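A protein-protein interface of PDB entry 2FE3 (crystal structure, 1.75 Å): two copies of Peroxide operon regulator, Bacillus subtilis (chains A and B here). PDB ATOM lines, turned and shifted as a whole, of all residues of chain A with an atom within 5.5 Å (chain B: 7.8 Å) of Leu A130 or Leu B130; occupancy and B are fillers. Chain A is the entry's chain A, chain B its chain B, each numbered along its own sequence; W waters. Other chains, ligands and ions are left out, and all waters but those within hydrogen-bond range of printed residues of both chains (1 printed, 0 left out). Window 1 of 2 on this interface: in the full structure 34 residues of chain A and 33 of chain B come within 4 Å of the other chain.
Printed residues of chain B within 4 Å of Leu A130: Leu B110 (3.7 Å), Val B113 (3.5 Å), Arg B129 (3.7 Å) and Leu B130 (3.99 Å). Of the printed residues of chain B, Glu A131 touches His B128 and Arg B129. Printed residues of chain A within 4 Å of Val B113: Leu A110 and Leu A130. Printed residues of chain A within 4 Å of Leu B130: Leu A110 (3.8 Å), Val A113 (3.7 Å), Arg A129 (3.6 Å) and Leu A130 (3.99 Å). The nearest printed residue of chain B that does not touch Leu A130 is His B128 (4.1 Å). The nearest printed residue of chain A that does not touch Leu B130 is His A128 (4.02 Å).
NH1 of Arg B129 lies close to NH1 of Arg A129 (2.7 Å). OE1 of Glu B131 lies within salt-bridge range of NH1 of Arg A129 (2.6 Å). The side-chain carboxylate (OE1) of Glu A131 lies within salt-bridge range of the guanidinium group (NH1) of Arg B129 (2.7 Å).
N of His A91 is in hydrogen-bond range of O of His A128 (3.1 Å). N of Leu A130 lies within hydrogen-bond range of O of His A91. The side-chain hydroxyl (OH) of Tyr A92 is in hydrogen-bond range of a ring nitrogen (NE2) of His A128. The backbone carbonyl oxygen (O) of His A93 is in hydrogen-bond range of the backbone NH (N) of Ile A132 (2.8 Å). O of His B91 is in hydrogen-bond range of N of Leu B130 (2.9 Å). The side-chain carboxylate (OE2) of Glu B114 is in hydrogen-bond range of a ring nitrogen (ND1) of His B128 (2.7 Å).
CD2 of Leu A110 touches CG2 of Val B113, 3.6 Å away. CD1 of Leu A110 touches CD1 of Leu B130 (3.8 Å). CG2 of Val A113 touches CD2 of Leu B110 (3.7 Å). CG1 of Val A113 touches CD2 of Leu B130, 3.7 Å away. CA of His A128 touches O of Glu B131 (3.1 Å). Leu B130 touches Arg A129. Leu A130 touches Leu B110 (CD1 to CD1, 3.7 Å). Arg B129 touches Leu A130. CD1 of Leu A130 touches CB of Leu B130, 3.99 Å away. C of Ile A132 touches O of His B127 (3.7 Å).
Leu A110 touches Val B113, and with the chains exchanged Val A113 touches Leu B110. His A128 touches Glu B131, and with the chains exchanged Glu A131 touches His B128. Arg A129 touches its own counterpart, Arg B129. Arg A129 touches Glu B131, and with the chains exchanged Glu A131 touches Arg B129. Positions printed for both chains: 91, 92, 93, 105, 110, 113, 128, 129, 130, 131 and 132.
Printed residues of chain B that touch a printed residue of chain A: Tyr B107, Leu B110, Val B113, Ala B117, His B127, His B128, Arg B129, Leu B130 and Glu B131. Hydrophobic or aromatic side chains of chain B within 4 Å of the printed part of chain A: Tyr B107, Leu B110, Val B113, Ala B117, His B128 and Leu B130.
Water W1 bridges the backbone carbonyl oxygen (O) of Arg B129 (3.2 Å) and the backbone carbonyl oxygen (O) of Arg A129 (3.2 Å).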
ATOM      1  N   HIS A  91       3.852 -23.069 -11.423  1.00  0.00           N
ATOM      2  CA  HIS A  91       2.485 -23.327 -10.958  1.00  0.00           C
ATOM      3  C   HIS A  91       2.334 -22.709  -9.587  1.00  0.00           C
ATOM      4  O   HIS A  91       3.255 -22.791  -8.779  1.00  0.00           O
ATOM      5  CB  HIS A  91       2.229 -24.842 -10.946  1.00  0.00           C
ATOM      6  CG  HIS A  91       2.127 -25.409 -12.327  1.00  0.00           C
ATOM      7  ND1 HIS A  91       1.060 -25.139 -13.153  1.00  0.00           N
ATOM      8  CD2 HIS A  91       2.989 -26.155 -13.054  1.00  0.00           C
ATOM      9  CE1 HIS A  91       1.256 -25.713 -14.329  1.00  0.00           C
ATOM     10  NE2 HIS A  91       2.414 -26.345 -14.292  1.00  0.00           N
ATOM     11  N   TYR A  92       1.166 -22.099  -9.352  1.00  0.00           N
ATOM     12  CA  TYR A  92       0.829 -21.493  -8.072  1.00  0.00           C
ATOM     13  C   TYR A  92      -0.539 -22.008  -7.684  1.00  0.00           C
ATOM     14  O   TYR A  92      -1.501 -21.918  -8.458  1.00  0.00           O
ATOM     15  CB  TYR A  92       0.801 -19.956  -8.162  1.00  0.00           C
ATOM     16  CG  TYR A  92       2.035 -19.386  -8.804  1.00  0.00           C
ATOM     17  CD1 TYR A  92       3.129 -19.020  -8.032  1.00  0.00           C
ATOM     18  CD2 TYR A  92       2.126 -19.237 -10.204  1.00  0.00           C
ATOM     19  CE1 TYR A  92       4.288 -18.515  -8.622  1.00  0.00           C
ATOM     20  CE2 TYR A  92       3.287 -18.711 -10.791  1.00  0.00           C
ATOM     21  CZ  TYR A  92       4.363 -18.367  -9.982  1.00  0.00           C
ATOM     22  OH  TYR A  92       5.520 -17.844 -10.539  1.00  0.00           O
ATOM     23  N   HIS A  93      -0.602 -22.550  -6.474  1.00  0.00           N
ATOM     24  CA  HIS A  93      -1.876 -23.153  -5.982  1.00  0.00           C
ATOM     25  C   HIS A  93      -2.137 -22.709  -4.565  1.00  0.00           C
ATOM     26  O   HIS A  93      -1.210 -22.658  -3.753  1.00  0.00           O
ATOM     27  CB  HIS A  93      -1.777 -24.677  -5.979  1.00  0.00           C
ATOM     28  CG  HIS A  93      -1.458 -25.260  -7.314  1.00  0.00           C
ATOM     29  ND1 HIS A  93      -0.294 -25.953  -7.568  1.00  0.00           N
ATOM     30  CD2 HIS A  93      -2.146 -25.234  -8.472  1.00  0.00           C
ATOM     31  CE1 HIS A  93      -0.290 -26.344  -8.832  1.00  0.00           C
ATOM     32  NE2 HIS A  93      -1.403 -25.918  -9.403  1.00  0.00           N
ATOM     33  N   PHE A 105      -3.692 -19.844  -9.043  1.00  0.00           N
ATOM     34  CA  PHE A 105      -3.601 -18.397  -9.279  1.00  0.00           C
ATOM     35  C   PHE A 105      -2.360 -18.078 -10.095  1.00  0.00           C
ATOM     36  O   PHE A 105      -1.535 -18.960 -10.314  1.00  0.00           O
ATOM     37  CB  PHE A 105      -3.652 -17.581  -7.976  1.00  0.00           C
ATOM     38  CG  PHE A 105      -2.507 -17.846  -7.017  1.00  0.00           C
ATOM     39  CD1 PHE A 105      -1.450 -16.919  -6.902  1.00  0.00           C
ATOM     40  CD2 PHE A 105      -2.513 -18.972  -6.197  1.00  0.00           C
ATOM     41  CE1 PHE A 105      -0.423 -17.141  -6.031  1.00  0.00           C
ATOM     42  CE2 PHE A 105      -1.475 -19.204  -5.295  1.00  0.00           C
ATOM     43  CZ  PHE A 105      -0.428 -18.275  -5.209  1.00  0.00           C
ATOM     44  N   LEU A 110       9.194 -15.755  -9.593  1.00  0.00           N
ATOM     45  CA  LEU A 110       9.878 -15.611  -8.311  1.00  0.00           C
ATOM     46  C   LEU A 110      11.376 -15.458  -8.545  1.00  0.00           C
ATOM     47  O   LEU A 110      12.182 -16.162  -7.920  1.00  0.00           O
ATOM     48  CB  LEU A 110       9.605 -16.832  -7.431  1.00  0.00           C
ATOM     49  CG  LEU A 110       8.121 -17.019  -7.013  1.00  0.00           C
ATOM     50  CD1 LEU A 110       7.928 -18.374  -6.310  1.00  0.00           C
ATOM     51  CD2 LEU A 110       7.662 -15.908  -6.118  1.00  0.00           C
ATOM     52  N   VAL A 113      13.887 -15.251  -5.479  1.00  0.00           N
ATOM     53  CA  VAL A 113      14.052 -16.502  -4.777  1.00  0.00           C
ATOM     54  C   VAL A 113      14.837 -17.512  -5.608  1.00  0.00           C
ATOM     55  O   VAL A 113      15.720 -18.185  -5.072  1.00  0.00           O
ATOM     56  CB  VAL A 113      12.695 -17.162  -4.386  1.00  0.00           C
ATOM     57  CG1 VAL A 113      12.965 -18.293  -3.385  1.00  0.00           C
ATOM     58  CG2 VAL A 113      11.748 -16.148  -3.815  1.00  0.00           C
ATOM     59  N   HIS A 128       9.232 -23.680 -10.993  1.00  0.00           N
ATOM     60  CA  HIS A 128       8.866 -23.883  -9.582  1.00  0.00           C
ATOM     61  C   HIS A 128       7.391 -24.165  -9.444  1.00  0.00           C
ATOM     62  O   HIS A 128       6.630 -23.855 -10.344  1.00  0.00           O
ATOM     63  CB  HIS A 128       9.236 -22.677  -8.697  1.00  0.00           C
ATOM     64  CG  HIS A 128       8.654 -21.367  -9.143  1.00  0.00           C
ATOM     65  ND1 HIS A 128       9.393 -20.431  -9.846  1.00  0.00           N
ATOM     66  CD2 HIS A 128       7.428 -20.826  -8.973  1.00  0.00           C
ATOM     67  CE1 HIS A 128       8.634 -19.377 -10.108  1.00  0.00           C
ATOM     68  NE2 HIS A 128       7.432 -19.597  -9.592  1.00  0.00           N
ATOM     69  N   ARG A 129       7.027 -24.747  -8.304  1.00  0.00           N
ATOM     70  CA  ARG A 129       5.644 -24.937  -7.912  1.00  0.00           C
ATOM     71  C   ARG A 129       5.555 -24.373  -6.483  1.00  0.00           C
ATOM     72  O   ARG A 129       6.362 -24.728  -5.601  1.00  0.00           O
ATOM     73  CB  ARG A 129       5.231 -26.420  -7.911  1.00  0.00           C
ATOM     74  CG  ARG A 129       3.742 -26.576  -7.550  1.00  0.00           C
ATOM     75  CD  ARG A 129       3.544 -27.607  -6.458  1.00  0.00           C
ATOM     76  NE  ARG A 129       3.550 -28.967  -6.972  1.00  0.00           N
ATOM     77  CZ  ARG A 129       3.908 -30.053  -6.279  1.00  0.00           C
ATOM     78  NH1 ARG A 129       4.325 -29.967  -5.028  1.00  0.00           N
ATOM     79  NH2 ARG A 129       3.862 -31.243  -6.856  1.00  0.00           N
ATOM     80  N   LEU A 130       4.619 -23.451  -6.300  1.00  0.00           N
ATOM     81  CA  LEU A 130       4.349 -22.866  -4.985  1.00  0.00           C
ATOM     82  C   LEU A 130       2.966 -23.327  -4.544  1.00  0.00           C
ATOM     83  O   LEU A 130       1.978 -23.145  -5.278  1.00  0.00           O
ATOM     84  CB  LEU A 130       4.408 -21.336  -5.039  1.00  0.00           C
ATOM     85  CG  LEU A 130       4.064 -20.615  -3.724  1.00  0.00           C
ATOM     86  CD1 LEU A 130       5.106 -20.892  -2.686  1.00  0.00           C
ATOM     87  CD2 LEU A 130       4.013 -19.096  -4.013  1.00  0.00           C
ATOM     88  N   GLU A 131       2.908 -23.886  -3.339  1.00  0.00           N
ATOM     89  CA  GLU A 131       1.652 -24.294  -2.722  1.00  0.00           C
ATOM     90  C   GLU A 131       1.472 -23.420  -1.507  1.00  0.00           C
ATOM     91  O   GLU A 131       2.357 -23.395  -0.629  1.00  0.00           O
ATOM     92  CB  GLU A 131       1.712 -25.759  -2.280  1.00  0.00           C
ATOM     93  CG  GLU A 131       1.757 -26.701  -3.459  1.00  0.00           C
ATOM     94  CD  GLU A 131       1.836 -28.165  -3.037  1.00  0.00           C
ATOM     95  OE1 GLU A 131       2.206 -28.451  -1.868  1.00  0.00           O
ATOM     96  OE2 GLU A 131       1.535 -29.035  -3.869  1.00  0.00           O
ATOM     97  N   ILE A 132       0.376 -22.662  -1.480  1.00  0.00           N
ATOM     98  CA  ILE A 132       0.060 -21.898  -0.291  1.00  0.00           C
ATOM     99  C   ILE A 132      -1.102 -22.558   0.446  1.00  0.00           C
ATOM    100  O   ILE A 132      -2.143 -22.797  -0.165  1.00  0.00           O
ATOM    101  CB  ILE A 132      -0.282 -20.454  -0.669  1.00  0.00           C
ATOM    102  CG1 ILE A 132       0.888 -19.837  -1.469  1.00  0.00           C
ATOM    103  CG2 ILE A 132      -0.621 -19.652   0.610  1.00  0.00           C
ATOM    104  CD1 ILE A 132       0.730 -18.337  -1.676  1.00  0.00           C
ATOM    105  N   ASP B  90       7.049 -22.763   7.041  1.00  0.00           N
ATOM    106  CA  ASP B  90       7.202 -22.811   5.584  1.00  0.00           C
ATOM    107  C   ASP B  90       8.340 -23.749   5.208  1.00  0.00           C
ATOM    108  O   ASP B  90       9.223 -24.044   6.032  1.00  0.00           O
ATOM    109  CB  ASP B  90       7.511 -21.423   5.042  1.00  0.00           C
ATOM    110  CG  ASP B  90       6.495 -20.404   5.480  1.00  0.00           C
ATOM    111  OD1 ASP B  90       5.298 -20.664   5.331  1.00  0.00           O
ATOM    112  OD2 ASP B  90       6.900 -19.358   6.007  1.00  0.00           O
ATOM    113  N   HIS B  91       8.337 -24.208   3.959  1.00  0.00           N
ATOM    114  CA  HIS B  91       9.413 -25.078   3.511  1.00  0.00           C
ATOM    115  C   HIS B  91       9.866 -24.661   2.125  1.00  0.00           C
ATOM    116  O   HIS B  91       9.044 -24.283   1.295  1.00  0.00           O
ATOM    117  CB  HIS B  91       8.950 -26.544   3.544  1.00  0.00           C
ATOM    118  CG  HIS B  91       8.735 -27.070   4.938  1.00  0.00           C
ATOM    119  ND1 HIS B  91       9.780 -27.440   5.759  1.00  0.00           N
ATOM    120  CD2 HIS B  91       7.607 -27.239   5.666  1.00  0.00           C
ATOM    121  CE1 HIS B  91       9.305 -27.836   6.929  1.00  0.00           C
ATOM    122  NE2 HIS B  91       7.987 -27.735   6.895  1.00  0.00           N
ATOM    123  N   TYR B  92      11.169 -24.709   1.897  1.00  0.00           N
ATOM    124  CA  TYR B  92      11.757 -24.401   0.593  1.00  0.00           C
ATOM    125  C   TYR B  92      12.678 -25.559   0.200  1.00  0.00           C
ATOM    126  O   TYR B  92      13.596 -25.915   0.952  1.00  0.00           O
ATOM    127  CB  TYR B  92      12.591 -23.104   0.676  1.00  0.00           C
ATOM    128  CG  TYR B  92      11.814 -21.967   1.276  1.00  0.00           C
ATOM    129  CD1 TYR B  92      11.059 -21.124   0.480  1.00  0.00           C
ATOM    130  CD2 TYR B  92      11.836 -21.736   2.653  1.00  0.00           C
ATOM    131  CE1 TYR B  92      10.310 -20.092   1.046  1.00  0.00           C
ATOM    132  CE2 TYR B  92      11.098 -20.719   3.208  1.00  0.00           C
ATOM    133  CZ  TYR B  92      10.345 -19.906   2.408  1.00  0.00           C
ATOM    134  OH  TYR B  92       9.636 -18.880   3.006  1.00  0.00           O
ATOM    135  N   HIS B  93      12.448 -26.100  -0.996  1.00  0.00           N
ATOM    136  CA  HIS B  93      13.206 -27.256  -1.481  1.00  0.00           C
ATOM    137  C   HIS B  93      13.675 -27.040  -2.939  1.00  0.00           C
ATOM    138  O   HIS B  93      12.916 -26.529  -3.760  1.00  0.00           O
ATOM    139  CB  HIS B  93      12.326 -28.518  -1.481  1.00  0.00           C
ATOM    140  CG  HIS B  93      11.625 -28.796  -0.190  1.00  0.00           C
ATOM    141  ND1 HIS B  93      12.294 -29.112   0.967  1.00  0.00           N
ATOM    142  CD2 HIS B  93      10.306 -28.850   0.112  1.00  0.00           C
ATOM    143  CE1 HIS B  93      11.422 -29.321   1.941  1.00  0.00           C
ATOM    144  NE2 HIS B  93      10.208 -29.166   1.447  1.00  0.00           N
ATOM    145  N   ALA B  94      14.920 -27.418  -3.230  1.00  0.00           N
ATOM    146  CA  ALA B  94      15.397 -27.524  -4.614  1.00  0.00           C
ATOM    147  C   ALA B  94      15.414 -29.002  -4.968  1.00  0.00           C
ATOM    148  O   ALA B  94      15.921 -29.817  -4.186  1.00  0.00           O
ATOM    149  CB  ALA B  94      16.793 -26.948  -4.760  1.00  0.00           C
ATOM    150  N   ILE B  95      14.877 -29.337  -6.137  1.00  0.00           N
ATOM    151  CA  ILE B  95      14.676 -30.721  -6.494  1.00  0.00           C
ATOM    152  C   ILE B  95      15.320 -30.980  -7.850  1.00  0.00           C
ATOM    153  O   ILE B  95      14.994 -30.301  -8.842  1.00  0.00           O
ATOM    154  CB  ILE B  95      13.170 -31.083  -6.565  1.00  0.00           C
ATOM    155  CG1 ILE B  95      12.458 -30.730  -5.247  1.00  0.00           C
ATOM    156  CG2 ILE B  95      13.006 -32.605  -6.909  1.00  0.00           C
ATOM    157  CD1 ILE B  95      10.966 -30.977  -5.259  1.00  0.00           C
ATOM    158  N   VAL B 103      17.280 -30.726  -1.891  1.00  0.00           N
ATOM    159  CA  VAL B 103      18.132 -29.923  -1.018  1.00  0.00           C
ATOM    160  C   VAL B 103      17.243 -28.846  -0.385  1.00  0.00           C
ATOM    161  O   VAL B 103      16.624 -28.046  -1.111  1.00  0.00           O
ATOM    162  CB  VAL B 103      19.271 -29.248  -1.821  1.00  0.00           C
ATOM    163  CG1 VAL B 103      20.045 -28.248  -0.957  1.00  0.00           C
ATOM    164  CG2 VAL B 103      20.226 -30.299  -2.400  1.00  0.00           C
ATOM    165  N   ASP B 104      17.173 -28.819   0.944  1.00  0.00           N
ATOM    166  CA  ASP B 104      16.391 -27.774   1.626  1.00  0.00           C
ATOM    167  C   ASP B 104      17.183 -26.468   1.682  1.00  0.00           C
ATOM    168  O   ASP B 104      18.425 -26.466   1.803  1.00  0.00           O
ATOM    169  CB  ASP B 104      16.007 -28.208   3.050  1.00  0.00           C
ATOM    170  CG  ASP B 104      15.261 -29.526   3.080  1.00  0.00           C
ATOM    171  OD1 ASP B 104      14.406 -29.771   2.207  1.00  0.00           O
ATOM    172  OD2 ASP B 104      15.553 -30.345   3.968  1.00  0.00           O
ATOM    173  N   PHE B 105      16.483 -25.347   1.569  1.00  0.00           N
ATOM    174  CA  PHE B 105      17.158 -24.078   1.740  1.00  0.00           C
ATOM    175  C   PHE B 105      16.287 -23.140   2.559  1.00  0.00           C
ATOM    176  O   PHE B 105      15.103 -23.424   2.804  1.00  0.00           O
ATOM    177  CB  PHE B 105      17.638 -23.469   0.409  1.00  0.00           C
ATOM    178  CG  PHE B 105      16.537 -23.061  -0.526  1.00  0.00           C
ATOM    179  CD1 PHE B 105      16.045 -21.740  -0.528  1.00  0.00           C
ATOM    180  CD2 PHE B 105      15.988 -23.988  -1.399  1.00  0.00           C
ATOM    181  CE1 PHE B 105      15.032 -21.365  -1.402  1.00  0.00           C
ATOM    182  CE2 PHE B 105      14.971 -23.621  -2.291  1.00  0.00           C
ATOM    183  CZ  PHE B 105      14.497 -22.304  -2.284  1.00  0.00           C
ATOM    184  N   TYR B 107      14.713 -19.278   3.089  1.00  0.00           N
ATOM    185  CA  TYR B 107      14.403 -17.950   2.548  1.00  0.00           C
ATOM    186  C   TYR B 107      13.477 -17.242   3.553  1.00  0.00           C
ATOM    187  O   TYR B 107      12.655 -17.909   4.179  1.00  0.00           O
ATOM    188  CB  TYR B 107      13.754 -18.082   1.151  1.00  0.00           C
ATOM    189  CG  TYR B 107      13.643 -16.781   0.398  1.00  0.00           C
ATOM    190  CD1 TYR B 107      14.730 -16.282  -0.331  1.00  0.00           C
ATOM    191  CD2 TYR B 107      12.461 -16.024   0.423  1.00  0.00           C
ATOM    192  CE1 TYR B 107      14.642 -15.086  -1.007  1.00  0.00           C
ATOM    193  CE2 TYR B 107      12.368 -14.812  -0.253  1.00  0.00           C
ATOM    194  CZ  TYR B 107      13.476 -14.348  -0.965  1.00  0.00           C
ATOM    195  OH  TYR B 107      13.408 -13.160  -1.634  1.00  0.00           O
ATOM    196  N   LEU B 110       7.583 -15.205   2.023  1.00  0.00           N
ATOM    197  CA  LEU B 110       7.112 -14.758   0.711  1.00  0.00           C
ATOM    198  C   LEU B 110       5.922 -13.852   0.909  1.00  0.00           C
ATOM    199  O   LEU B 110       4.869 -14.066   0.291  1.00  0.00           O
ATOM    200  CB  LEU B 110       6.712 -15.950  -0.169  1.00  0.00           C
ATOM    201  CG  LEU B 110       7.824 -16.904  -0.593  1.00  0.00           C
ATOM    202  CD1 LEU B 110       7.224 -18.161  -1.269  1.00  0.00           C
ATOM    203  CD2 LEU B 110       8.803 -16.171  -1.510  1.00  0.00           C
ATOM    204  N   VAL B 113       3.881 -12.383  -2.153  1.00  0.00           N
ATOM    205  CA  VAL B 113       3.129 -13.424  -2.819  1.00  0.00           C
ATOM    206  C   VAL B 113       1.915 -13.872  -1.986  1.00  0.00           C
ATOM    207  O   VAL B 113       0.807 -13.985  -2.520  1.00  0.00           O
ATOM    208  CB  VAL B 113       4.006 -14.675  -3.147  1.00  0.00           C
ATOM    209  CG1 VAL B 113       3.153 -15.707  -3.863  1.00  0.00           C
ATOM    210  CG2 VAL B 113       5.180 -14.272  -4.015  1.00  0.00           C
ATOM    211  N   GLU B 114       2.134 -14.139  -0.706  1.00  0.00           N
ATOM    212  CA  GLU B 114       1.036 -14.530   0.203  1.00  0.00           C
ATOM    213  C   GLU B 114      -0.062 -13.465   0.235  1.00  0.00           C
ATOM    214  O   GLU B 114      -1.251 -13.785   0.201  1.00  0.00           O
ATOM    215  CB  GLU B 114       1.566 -14.783   1.615  1.00  0.00           C
ATOM    216  CG  GLU B 114       2.361 -16.092   1.739  1.00  0.00           C
ATOM    217  CD  GLU B 114       2.566 -16.514   3.192  1.00  0.00           C
ATOM    218  OE1 GLU B 114       2.304 -15.684   4.095  1.00  0.00           O
ATOM    219  OE2 GLU B 114       2.971 -17.680   3.440  1.00  0.00           O
ATOM    220  N   ALA B 117      -1.867 -13.564  -3.134  1.00  0.00           N
ATOM    221  CA  ALA B 117      -2.642 -14.811  -3.219  1.00  0.00           C
ATOM    222  C   ALA B 117      -3.925 -14.740  -2.395  1.00  0.00           C
ATOM    223  O   ALA B 117      -4.983 -15.161  -2.844  1.00  0.00           O
ATOM    224  CB  ALA B 117      -1.794 -16.011  -2.762  1.00  0.00           C
ATOM    225  N   HIS B 127       0.643 -20.996   5.623  1.00  0.00           N
ATOM    226  CA  HIS B 127       2.046 -21.268   5.334  1.00  0.00           C
ATOM    227  C   HIS B 127       2.210 -21.745   3.897  1.00  0.00           C
ATOM    228  O   HIS B 127       1.242 -21.906   3.174  1.00  0.00           O
ATOM    229  CB  HIS B 127       2.599 -22.330   6.278  1.00  0.00           C
ATOM    230  CG  HIS B 127       1.869 -23.636   6.199  1.00  0.00           C
ATOM    231  ND1 HIS B 127       0.610 -23.817   6.731  1.00  0.00           N
ATOM    232  CD2 HIS B 127       2.204 -24.810   5.615  1.00  0.00           C
ATOM    233  CE1 HIS B 127       0.216 -25.058   6.508  1.00  0.00           C
ATOM    234  NE2 HIS B 127       1.155 -25.672   5.814  1.00  0.00           N
ATOM    235  N   HIS B 128       3.448 -21.951   3.479  1.00  0.00           N
ATOM    236  CA  HIS B 128       3.667 -22.341   2.086  1.00  0.00           C
ATOM    237  C   HIS B 128       4.792 -23.364   1.931  1.00  0.00           C
ATOM    238  O   HIS B 128       5.617 -23.519   2.824  1.00  0.00           O
ATOM    239  CB  HIS B 128       3.919 -21.123   1.195  1.00  0.00           C
ATOM    240  CG  HIS B 128       5.084 -20.290   1.628  1.00  0.00           C
ATOM    241  ND1 HIS B 128       4.934 -19.111   2.336  1.00  0.00           N
ATOM    242  CD2 HIS B 128       6.418 -20.482   1.487  1.00  0.00           C
ATOM    243  CE1 HIS B 128       6.128 -18.604   2.587  1.00  0.00           C
ATOM    244  NE2 HIS B 128       7.046 -19.427   2.100  1.00  0.00           N
ATOM    245  N   ARG B 129       4.795 -24.063   0.790  1.00  0.00           N
ATOM    246  CA  ARG B 129       5.876 -24.967   0.416  1.00  0.00           C
ATOM    247  C   ARG B 129       6.250 -24.555  -0.996  1.00  0.00           C
ATOM    248  O   ARG B 129       5.381 -24.497  -1.879  1.00  0.00           O
ATOM    249  CB  ARG B 129       5.401 -26.431   0.383  1.00  0.00           C
ATOM    250  CG  ARG B 129       6.460 -27.371  -0.179  1.00  0.00           C
ATOM    251  CD  ARG B 129       5.797 -28.396  -1.146  1.00  0.00           C
ATOM    252  NE  ARG B 129       5.131 -29.486  -0.459  1.00  0.00           N
ATOM    253  CZ  ARG B 129       4.361 -30.405  -1.052  1.00  0.00           C
ATOM    254  NH1 ARG B 129       4.111 -30.363  -2.356  1.00  0.00           N
ATOM    255  NH2 ARG B 129       3.816 -31.365  -0.325  1.00  0.00           N
ATOM    256  N   LEU B 130       7.521 -24.215  -1.194  1.00  0.00           N
ATOM    257  CA  LEU B 130       8.003 -23.830  -2.521  1.00  0.00           C
ATOM    258  C   LEU B 130       8.949 -24.927  -2.970  1.00  0.00           C
ATOM    259  O   LEU B 130       9.900 -25.264  -2.244  1.00  0.00           O
ATOM    260  CB  LEU B 130       8.754 -22.500  -2.456  1.00  0.00           C
ATOM    261  CG  LEU B 130       9.451 -22.072  -3.745  1.00  0.00           C
ATOM    262  CD1 LEU B 130       8.454 -21.845  -4.846  1.00  0.00           C
ATOM    263  CD2 LEU B 130      10.253 -20.786  -3.478  1.00  0.00           C
ATOM    264  N   GLU B 131       8.660 -25.496  -4.136  1.00  0.00           N
ATOM    265  CA  GLU B 131       9.573 -26.452  -4.761  1.00  0.00           C
ATOM    266  C   GLU B 131      10.181 -25.839  -6.014  1.00  0.00           C
ATOM    267  O   GLU B 131       9.461 -25.402  -6.914  1.00  0.00           O
ATOM    268  CB  GLU B 131       8.822 -27.714  -5.135  1.00  0.00           C
ATOM    269  CG  GLU B 131       8.239 -28.410  -3.929  1.00  0.00           C
ATOM    270  CD  GLU B 131       7.479 -29.665  -4.323  1.00  0.00           C
ATOM    271  OE1 GLU B 131       6.902 -29.684  -5.432  1.00  0.00           O
ATOM    272  OE2 GLU B 131       7.463 -30.619  -3.520  1.00  0.00           O
ATOM    273  N   ILE B 132      11.502 -25.794  -6.052  1.00  0.00           N
ATOM    274  CA  ILE B 132      12.189 -25.305  -7.231  1.00  0.00           C
ATOM    275  C   ILE B 132      12.835 -26.476  -7.925  1.00  0.00           C
ATOM    276  O   ILE B 132      13.607 -27.202  -7.309  1.00  0.00           O
ATOM    277  CB  ILE B 132      13.245 -24.224  -6.885  1.00  0.00           C
ATOM    278  CG1 ILE B 132      12.566 -23.081  -6.099  1.00  0.00           C
ATOM    279  CG2 ILE B 132      13.878 -23.713  -8.204  1.00  0.00           C
ATOM    280  CD1 ILE B 132      13.438 -21.863  -5.813  1.00  0.00           C
ATOM    281  N   TYR B 133      12.509 -26.637  -9.206  1.00  0.00           N
ATOM    282  CA  TYR B 133      12.993 -27.757  -9.992  1.00  0.00           C
ATOM    283  C   TYR B 133      14.140 -27.296 -10.849  1.00  0.00           C
ATOM    284  O   TYR B 133      14.103 -26.200 -11.424  1.00  0.00           O
ATOM    285  CB  TYR B 133      11.894 -28.313 -10.877  1.00  0.00           C
ATOM    286  CG  TYR B 133      10.779 -28.885 -10.045  1.00  0.00           C
ATOM    287  CD1 TYR B 133       9.650 -28.110  -9.713  1.00  0.00           C
ATOM    288  CD2 TYR B 133      10.868 -30.191  -9.571  1.00  0.00           C
ATOM    289  CE1 TYR B 133       8.635 -28.655  -8.898  1.00  0.00           C
ATOM    290  CE2 TYR B 133       9.877 -30.739  -8.783  1.00  0.00           C
ATOM    291  CZ  TYR B 133       8.774 -29.979  -8.443  1.00  0.00           C
ATOM    292  OH  TYR B 133       7.808 -30.586  -7.641  1.00  0.00           O
HETATM  293  O   HOH W   1       5.206 -27.024  -3.752  1.00  0.00           O
